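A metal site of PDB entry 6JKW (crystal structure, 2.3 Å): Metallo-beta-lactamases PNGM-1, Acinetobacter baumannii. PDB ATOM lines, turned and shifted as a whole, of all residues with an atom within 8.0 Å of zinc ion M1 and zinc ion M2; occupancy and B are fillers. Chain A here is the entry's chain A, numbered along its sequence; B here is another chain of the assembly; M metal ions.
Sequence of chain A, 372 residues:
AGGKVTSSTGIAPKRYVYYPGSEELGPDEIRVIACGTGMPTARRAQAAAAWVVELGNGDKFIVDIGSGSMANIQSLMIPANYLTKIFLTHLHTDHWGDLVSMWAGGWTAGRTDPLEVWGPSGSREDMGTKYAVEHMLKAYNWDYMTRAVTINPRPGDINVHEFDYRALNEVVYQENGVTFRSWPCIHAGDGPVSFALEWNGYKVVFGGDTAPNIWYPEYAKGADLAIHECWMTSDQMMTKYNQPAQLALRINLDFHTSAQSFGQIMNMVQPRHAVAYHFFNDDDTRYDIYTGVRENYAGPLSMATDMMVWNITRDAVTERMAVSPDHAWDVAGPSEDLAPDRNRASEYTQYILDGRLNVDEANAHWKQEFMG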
ATOM      1  N   GLY A  38     -23.238   1.469 -11.277  1.00  0.00           N
ATOM      2  CA  GLY A  38     -22.435   1.822 -12.436  1.00  0.00           C
ATOM      3  C   GLY A  38     -22.822   1.099 -13.702  1.00  0.00           C
ATOM      4  O   GLY A  38     -23.982   0.953 -13.970  1.00  0.00           O
ATOM      5  N   MET A  39     -21.815   0.651 -14.439  1.00  0.00           N
ATOM      6  CA  MET A  39     -21.874   0.356 -15.886  1.00  0.00           C
ATOM      7  C   MET A  39     -21.103  -0.913 -16.065  1.00  0.00           C
ATOM      8  O   MET A  39     -20.509  -1.408 -15.092  1.00  0.00           O
ATOM      9  CB  MET A  39     -21.038   1.397 -16.610  1.00  0.00           C
ATOM     10  CG  MET A  39     -21.560   2.825 -16.554  1.00  0.00           C
ATOM     11  SD  MET A  39     -23.055   3.061 -17.820  1.00  0.00           S
ATOM     12  CE  MET A  39     -22.297   2.442 -19.541  1.00  0.00           C
ATOM     13  N   PRO A  40     -21.033  -1.446 -17.306  1.00  0.00           N
ATOM     14  CA  PRO A  40     -20.168  -2.639 -17.473  1.00  0.00           C
ATOM     15  C   PRO A  40     -18.663  -2.330 -17.540  1.00  0.00           C
ATOM     16  O   PRO A  40     -17.854  -3.239 -17.704  1.00  0.00           O
ATOM     17  CB  PRO A  40     -20.675  -3.237 -18.794  1.00  0.00           C
ATOM     18  CG  PRO A  40     -21.287  -2.089 -19.514  1.00  0.00           C
ATOM     19  CD  PRO A  40     -21.913  -1.243 -18.452  1.00  0.00           C
ATOM     20  N   ALA A  48     -20.655  -2.297 -10.207  1.00  0.00           N
ATOM     21  CA  ALA A  48     -21.784  -2.542 -11.114  1.00  0.00           C
ATOM     22  C   ALA A  48     -23.031  -2.866 -10.288  1.00  0.00           C
ATOM     23  O   ALA A  48     -22.912  -3.275  -9.117  1.00  0.00           O
ATOM     24  CB  ALA A  48     -21.482  -3.690 -12.046  1.00  0.00           C
ATOM     25  N   ALA A  49     -24.189  -2.781 -10.905  1.00  0.00           N
ATOM     26  CA  ALA A  49     -25.461  -2.850 -10.199  1.00  0.00           C
ATOM     27  C   ALA A  49     -25.585  -3.928  -9.110  1.00  0.00           C
ATOM     28  O   ALA A  49     -25.287  -5.106  -9.358  1.00  0.00           O
ATOM     29  CB  ALA A  49     -26.561  -3.074 -11.204  1.00  0.00           C
ATOM     30  N   ASP A  64     -29.616  -8.146  -8.012  1.00  0.00           N
ATOM     31  CA  ASP A  64     -28.414  -7.975  -8.848  1.00  0.00           C
ATOM     32  C   ASP A  64     -27.164  -7.987  -8.021  1.00  0.00           C
ATOM     33  O   ASP A  64     -27.160  -7.537  -6.926  1.00  0.00           O
ATOM     34  CB  ASP A  64     -28.531  -6.730  -9.794  1.00  0.00           C
ATOM     35  CG  ASP A  64     -29.525  -6.943 -10.922  1.00  0.00           C
ATOM     36  OD1 ASP A  64     -29.913  -8.148 -11.126  1.00  0.00           O
ATOM     37  OD2 ASP A  64     -29.963  -5.938 -11.558  1.00  0.00           O
ATOM     38  N   THR A  89     -32.071  -9.429 -12.297  1.00  0.00           N
ATOM     39  CA  THR A  89     -32.877  -8.833 -13.345  1.00  0.00           C
ATOM     40  C   THR A  89     -32.538  -9.362 -14.740  1.00  0.00           C
ATOM     41  O   THR A  89     -33.403  -9.505 -15.578  1.00  0.00           O
ATOM     42  CB  THR A  89     -32.693  -7.329 -13.424  1.00  0.00           C
ATOM     43  OG1 THR A  89     -31.324  -7.015 -13.712  1.00  0.00           O
ATOM     44  CG2 THR A  89     -33.256  -6.634 -12.191  1.00  0.00           C
ATOM     45  N   HIS A  90     -31.261  -9.588 -15.003  1.00  0.00           N
ATOM     46  CA  HIS A  90     -30.826 -10.172 -16.273  1.00  0.00           C
ATOM     47  C   HIS A  90     -29.418 -10.607 -16.221  1.00  0.00           C
ATOM     48  O   HIS A  90     -28.759 -10.391 -15.235  1.00  0.00           O
ATOM     49  CB  HIS A  90     -31.017  -9.213 -17.439  1.00  0.00           C
ATOM     50  CG  HIS A  90     -30.243  -7.938 -17.327  1.00  0.00           C
ATOM     51  ND1 HIS A  90     -30.406  -7.059 -16.278  1.00  0.00           N
ATOM     52  CD2 HIS A  90     -29.357  -7.369 -18.160  1.00  0.00           C
ATOM     53  CE1 HIS A  90     -29.635  -6.005 -16.470  1.00  0.00           C
ATOM     54  NE2 HIS A  90     -29.006  -6.164 -17.616  1.00  0.00           N
ATOM     55  N   LEU A  91     -28.921 -11.161 -17.313  1.00  0.00           N
ATOM     56  CA  LEU A  91     -27.724 -11.974 -17.288  1.00  0.00           C
ATOM     57  C   LEU A  91     -26.494 -11.315 -17.888  1.00  0.00           C
ATOM     58  O   LEU A  91     -25.503 -11.965 -18.234  1.00  0.00           O
ATOM     59  CB  LEU A  91     -28.082 -13.325 -17.947  1.00  0.00           C
ATOM     60  CG  LEU A  91     -29.145 -14.184 -17.233  1.00  0.00           C
ATOM     61  CD1 LEU A  91     -29.368 -15.440 -18.052  1.00  0.00           C
ATOM     62  CD2 LEU A  91     -28.669 -14.624 -15.850  1.00  0.00           C
ATOM     63  N   HIS A  92     -26.514  -9.984 -17.944  1.00  0.00           N
ATOM     64  CA  HIS A  92     -25.284  -9.248 -18.237  1.00  0.00           C
ATOM     65  C   HIS A  92     -24.350  -9.346 -17.066  1.00  0.00           C
ATOM     66  O   HIS A  92     -24.776  -9.309 -15.933  1.00  0.00           O
ATOM     67  CB  HIS A  92     -25.515  -7.756 -18.460  1.00  0.00           C
ATOM     68  CG  HIS A  92     -25.865  -7.373 -19.851  1.00  0.00           C
ATOM     69  ND1 HIS A  92     -26.850  -6.473 -20.131  1.00  0.00           N
ATOM     70  CD2 HIS A  92     -25.318  -7.715 -21.032  1.00  0.00           C
ATOM     71  CE1 HIS A  92     -26.938  -6.304 -21.446  1.00  0.00           C
ATOM     72  NE2 HIS A  92     -26.027  -7.068 -22.009  1.00  0.00           N
ATOM     73  N   THR A  93     -23.068  -9.387 -17.376  1.00  0.00           N
ATOM     74  CA  THR A  93     -21.985  -9.420 -16.404  1.00  0.00           C
ATOM     75  C   THR A  93     -22.089  -8.308 -15.355  1.00  0.00           C
ATOM     76  O   THR A  93     -21.811  -8.545 -14.175  1.00  0.00           O
ATOM     77  CB  THR A  93     -20.599  -9.374 -17.125  1.00  0.00           C
ATOM     78  OG1 THR A  93     -20.329  -8.058 -17.569  1.00  0.00           O
ATOM     79  CG2 THR A  93     -20.607 -10.302 -18.360  1.00  0.00           C
ATOM     80  N   ASP A  94     -22.503  -7.117 -15.724  1.00  0.00           N
ATOM     81  CA  ASP A  94     -22.551  -6.050 -14.737  1.00  0.00           C
ATOM     82  C   ASP A  94     -23.778  -6.177 -13.820  1.00  0.00           C
ATOM     83  O   ASP A  94     -24.067  -5.278 -12.985  1.00  0.00           O
ATOM     84  CB  ASP A  94     -22.480  -4.684 -15.426  1.00  0.00           C
ATOM     85  CG  ASP A  94     -23.584  -4.467 -16.401  1.00  0.00           C
ATOM     86  OD1 ASP A  94     -24.413  -3.492 -16.258  1.00  0.00           O
ATOM     87  OD2 ASP A  94     -23.624  -5.302 -17.325  1.00  0.00           O
ATOM     88  N   HIS A  95     -24.525  -7.277 -13.955  1.00  0.00           N
ATOM     89  CA  HIS A  95     -25.617  -7.575 -13.046  1.00  0.00           C
ATOM     90  C   HIS A  95     -25.489  -8.873 -12.294  1.00  0.00           C
ATOM     91  O   HIS A  95     -26.179  -9.035 -11.292  1.00  0.00           O
ATOM     92  CB  HIS A  95     -26.906  -7.552 -13.815  1.00  0.00           C
ATOM     93  CG  HIS A  95     -27.283  -6.167 -14.175  1.00  0.00           C
ATOM     94  ND1 HIS A  95     -28.227  -5.450 -13.471  1.00  0.00           N
ATOM     95  CD2 HIS A  95     -26.739  -5.310 -15.059  1.00  0.00           C
ATOM     96  CE1 HIS A  95     -28.293  -4.226 -13.968  1.00  0.00           C
ATOM     97  NE2 HIS A  95     -27.381  -4.120 -14.899  1.00  0.00           N
ATOM     98  N   HIS A 187     -34.327  -4.912 -23.673  1.00  0.00           N
ATOM     99  CA  HIS A 187     -32.911  -4.681 -23.470  1.00  0.00           C
ATOM    100  C   HIS A 187     -32.064  -5.817 -24.041  1.00  0.00           C
ATOM    101  O   HIS A 187     -32.017  -6.903 -23.468  1.00  0.00           O
ATOM    102  CB  HIS A 187     -32.730  -4.592 -21.983  1.00  0.00           C
ATOM    103  CG  HIS A 187     -31.321  -4.505 -21.522  1.00  0.00           C
ATOM    104  ND1 HIS A 187     -30.582  -3.347 -21.588  1.00  0.00           N
ATOM    105  CD2 HIS A 187     -30.548  -5.415 -20.904  1.00  0.00           C
ATOM    106  CE1 HIS A 187     -29.385  -3.576 -21.094  1.00  0.00           C
ATOM    107  NE2 HIS A 187     -29.354  -4.816 -20.631  1.00  0.00           N
ATOM    108  N   ALA A 188     -31.437  -5.568 -25.206  1.00  0.00           N
ATOM    109  CA  ALA A 188     -30.454  -6.455 -25.871  1.00  0.00           C
ATOM    110  C   ALA A 188     -31.058  -7.713 -26.533  1.00  0.00           C
ATOM    111  O   ALA A 188     -30.573  -8.144 -27.580  1.00  0.00           O
ATOM    112  CB  ALA A 188     -29.353  -6.859 -24.906  1.00  0.00           C
ATOM    113  N   PRO A 192     -34.494 -10.144 -19.929  1.00  0.00           N
ATOM    114  CA  PRO A 192     -34.450  -9.126 -18.855  1.00  0.00           C
ATOM    115  C   PRO A 192     -35.813  -8.792 -18.336  1.00  0.00           C
ATOM    116  O   PRO A 192     -36.764  -8.796 -19.125  1.00  0.00           O
ATOM    117  CB  PRO A 192     -33.798  -7.930 -19.554  1.00  0.00           C
ATOM    118  CG  PRO A 192     -32.938  -8.553 -20.596  1.00  0.00           C
ATOM    119  CD  PRO A 192     -33.763  -9.690 -21.116  1.00  0.00           C
ATOM    120  N   GLY A 208     -34.014  -2.734 -13.155  1.00  0.00           N
ATOM    121  CA  GLY A 208     -33.109  -3.428 -14.080  1.00  0.00           C
ATOM    122  C   GLY A 208     -32.678  -2.531 -15.250  1.00  0.00           C
ATOM    123  O   GLY A 208     -32.497  -1.337 -15.089  1.00  0.00           O
ATOM    124  N   ASP A 209     -32.488  -3.117 -16.434  1.00  0.00           N
ATOM    125  CA  ASP A 209     -32.073  -2.331 -17.608  1.00  0.00           C
ATOM    126  C   ASP A 209     -33.189  -2.464 -18.606  1.00  0.00           C
ATOM    127  O   ASP A 209     -33.688  -3.583 -18.838  1.00  0.00           O
ATOM    128  CB  ASP A 209     -30.865  -2.907 -18.311  1.00  0.00           C
ATOM    129  CG  ASP A 209     -29.563  -2.741 -17.550  1.00  0.00           C
ATOM    130  OD1 ASP A 209     -29.523  -2.078 -16.494  1.00  0.00           O
ATOM    131  OD2 ASP A 209     -28.541  -3.329 -18.039  1.00  0.00           O
ATOM    132  N   THR A 210     -33.529  -1.340 -19.224  1.00  0.00           N
ATOM    133  CA  THR A 210     -34.566  -1.324 -20.251  1.00  0.00           C
ATOM    134  C   THR A 210     -34.615   0.025 -21.000  1.00  0.00           C
ATOM    135  O   THR A 210     -34.314   1.094 -20.411  1.00  0.00           O
ATOM    136  CB  THR A 210     -35.946  -1.611 -19.607  1.00  0.00           C
ATOM    137  OG1 THR A 210     -36.939  -1.852 -20.630  1.00  0.00           O
ATOM    138  CG2 THR A 210     -36.344  -0.470 -18.639  1.00  0.00           C
ATOM    139  N   GLU A 229     -33.350   2.649 -14.847  1.00  0.00           N
ATOM    140  CA  GLU A 229     -32.240   3.093 -15.656  1.00  0.00           C
ATOM    141  C   GLU A 229     -32.478   4.515 -16.189  1.00  0.00           C
ATOM    142  O   GLU A 229     -33.579   4.875 -16.597  1.00  0.00           O
ATOM    143  CB  GLU A 229     -32.023   2.069 -16.785  1.00  0.00           C
ATOM    144  CG  GLU A 229     -32.040   2.618 -18.215  1.00  0.00           C
ATOM    145  CD  GLU A 229     -31.341   1.715 -19.238  1.00  0.00           C
ATOM    146  OE1 GLU A 229     -31.451   0.454 -19.173  1.00  0.00           O
ATOM    147  OE2 GLU A 229     -30.691   2.275 -20.107  1.00  0.00           O
ATOM    148  N   TRP A 231     -29.994   6.976 -18.627  1.00  0.00           N
ATOM    149  CA  TRP A 231     -28.688   6.895 -19.309  1.00  0.00           C
ATOM    150  C   TRP A 231     -27.997   8.227 -19.442  1.00  0.00           C
ATOM    151  O   TRP A 231     -28.613   9.262 -19.297  1.00  0.00           O
ATOM    152  CB  TRP A 231     -28.810   6.227 -20.670  1.00  0.00           C
ATOM    153  CG  TRP A 231     -27.569   5.575 -21.194  1.00  0.00           C
ATOM    154  CD1 TRP A 231     -26.760   6.048 -22.170  1.00  0.00           C
ATOM    155  CD2 TRP A 231     -27.035   4.296 -20.840  1.00  0.00           C
ATOM    156  NE1 TRP A 231     -25.734   5.173 -22.424  1.00  0.00           N
ATOM    157  CE2 TRP A 231     -25.902   4.077 -21.630  1.00  0.00           C
ATOM    158  CE3 TRP A 231     -27.419   3.321 -19.913  1.00  0.00           C
ATOM    159  CZ2 TRP A 231     -25.113   2.907 -21.527  1.00  0.00           C
ATOM    160  CZ3 TRP A 231     -26.628   2.145 -19.797  1.00  0.00           C
ATOM    161  CH2 TRP A 231     -25.497   1.960 -20.610  1.00  0.00           C
ATOM    162  N   HIS A 256     -31.668   2.821 -24.709  1.00  0.00           N
ATOM    163  CA  HIS A 256     -31.696   3.212 -23.321  1.00  0.00           C
ATOM    164  C   HIS A 256     -32.787   4.187 -23.008  1.00  0.00           C
ATOM    165  O   HIS A 256     -33.438   4.714 -23.885  1.00  0.00           O
ATOM    166  CB  HIS A 256     -30.337   3.777 -22.892  1.00  0.00           C
ATOM    167  CG  HIS A 256     -29.226   2.773 -23.032  1.00  0.00           C
ATOM    168  ND1 HIS A 256     -29.018   1.767 -22.114  1.00  0.00           N
ATOM    169  CD2 HIS A 256     -28.332   2.577 -24.034  1.00  0.00           C
ATOM    170  CE1 HIS A 256     -28.024   0.998 -22.534  1.00  0.00           C
ATOM    171  NE2 HIS A 256     -27.588   1.472 -23.686  1.00  0.00           N
ATOM    172  N   TYR A 277     -30.426   5.511 -11.761  1.00  0.00           N
ATOM    173  CA  TYR A 277     -29.102   4.894 -11.616  1.00  0.00           C
ATOM    174  C   TYR A 277     -28.605   4.461 -12.959  1.00  0.00           C
ATOM    175  O   TYR A 277     -29.308   4.597 -13.943  1.00  0.00           O
ATOM    176  CB  TYR A 277     -29.171   3.655 -10.629  1.00  0.00           C
ATOM    177  CG  TYR A 277     -29.512   2.315 -11.277  1.00  0.00           C
ATOM    178  CD1 TYR A 277     -30.739   2.093 -11.880  1.00  0.00           C
ATOM    179  CD2 TYR A 277     -28.602   1.276 -11.282  1.00  0.00           C
ATOM    180  CE1 TYR A 277     -31.032   0.866 -12.483  1.00  0.00           C
ATOM    181  CE2 TYR A 277     -28.878   0.044 -11.898  1.00  0.00           C
ATOM    182  CZ  TYR A 277     -30.110  -0.162 -12.469  1.00  0.00           C
ATOM    183  OH  TYR A 277     -30.404  -1.410 -13.050  1.00  0.00           O
ATOM    184  N   HIS A 278     -27.425   3.839 -12.935  1.00  0.00           N
ATOM    185  CA  HIS A 278     -26.779   3.178 -14.094  1.00  0.00           C
ATOM    186  C   HIS A 278     -26.137   4.148 -15.043  1.00  0.00           C
ATOM    187  O   HIS A 278     -26.015   3.909 -16.239  1.00  0.00           O
ATOM    188  CB  HIS A 278     -27.780   2.285 -14.802  1.00  0.00           C
ATOM    189  CG  HIS A 278     -27.174   1.060 -15.416  1.00  0.00           C
ATOM    190  ND1 HIS A 278     -26.320   1.096 -16.490  1.00  0.00           N
ATOM    191  CD2 HIS A 278     -27.389  -0.251 -15.161  1.00  0.00           C
ATOM    192  CE1 HIS A 278     -26.026  -0.127 -16.870  1.00  0.00           C
ATOM    193  NE2 HIS A 278     -26.661  -0.969 -16.076  1.00  0.00           N
ATOM    194  N   TRP B 142     -25.924 -15.714 -22.687  1.00  0.00           N
ATOM    195  CA  TRP B 142     -26.964 -14.727 -23.019  1.00  0.00           C
ATOM    196  C   TRP B 142     -26.354 -13.382 -23.410  1.00  0.00           C
ATOM    197  O   TRP B 142     -26.800 -12.735 -24.334  1.00  0.00           O
ATOM    198  CB  TRP B 142     -27.917 -14.516 -21.842  1.00  0.00           C
ATOM    199  CG  TRP B 142     -29.013 -13.566 -22.150  1.00  0.00           C
ATOM    200  CD1 TRP B 142     -30.218 -13.868 -22.731  1.00  0.00           C
ATOM    201  CD2 TRP B 142     -29.008 -12.155 -21.943  1.00  0.00           C
ATOM    202  NE1 TRP B 142     -30.944 -12.721 -22.903  1.00  0.00           N
ATOM    203  CE2 TRP B 142     -30.238 -11.658 -22.422  1.00  0.00           C
ATOM    204  CE3 TRP B 142     -28.070 -11.256 -21.413  1.00  0.00           C
ATOM    205  CZ2 TRP B 142     -30.556 -10.339 -22.413  1.00  0.00           C
ATOM    206  CZ3 TRP B 142     -28.412  -9.919 -21.382  1.00  0.00           C
ATOM    207  CH2 TRP B 142     -29.669  -9.477 -21.868  1.00  0.00           C
ATOM    208  N   ASP B 143     -25.384 -12.951 -22.625  1.00  0.00           N
ATOM    209  CA  ASP B 143     -24.645 -11.705 -22.792  1.00  0.00           C
ATOM    210  C   ASP B 143     -23.875 -11.807 -24.108  1.00  0.00           C
ATOM    211  O   ASP B 143     -23.900 -10.890 -24.909  1.00  0.00           O
ATOM    212  CB  ASP B 143     -23.703 -11.545 -21.546  1.00  0.00           C
ATOM    213  CG  ASP B 143     -22.917 -10.200 -21.506  1.00  0.00           C
ATOM    214  OD1 ASP B 143     -22.278  -9.861 -22.543  1.00  0.00           O
ATOM    215  OD2 ASP B 143     -22.884  -9.542 -20.396  1.00  0.00           O
HETATM  216 ZN    ZN M   1     -27.771  -4.878 -19.129  1.00  0.00          ZN
HETATM  217 ZN    ZN M   2     -26.724  -3.036 -16.952  1.00  0.00          ZN
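A ring nitrogen (ND1) of His 90 lies within hydrogen-bond range of the side-chain hydroxyl (OG1) of Thr 89.
The backbone NH (N) of Ala 49 is in hydrogen-bond range of the backbone carbonyl oxygen (O) of Asp 94.
ND1 of His 278 sits at hydrogen-bond distance from O of Gly 38, at 3.4 Å.
ND1 of His 95 sits at hydrogen-bond distance from OD2 of Asp 64 (2.6 Å).
ND1 of His 95 is in hydrogen-bond range of OG1 of Thr 89 (3.5 Å).
Of the 26 residues printed, 5 come within 4 Å of zinc ion M2.
The nearest printed residue that does not touch zinc ion M2 is His 92 (4.7 Å).
Zinc ion M1 is bound by the side-chain carboxylate (OD2) of Asp 209 (2.0 Å), a ring nitrogen (ND1) of His 92 (2.1 Å), a ring nitrogen (NE2) of His 187 (2.2 Å) and a ring nitrogen (NE2) of His 90 (2.3 Å).
Zinc ion M1 has four donor atoms within binding distance.
Zinc ion M2 is bound by OD2 of Asp 209, NE2 of His 278, NE2 of His 95 and OD1 of Asp 94.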
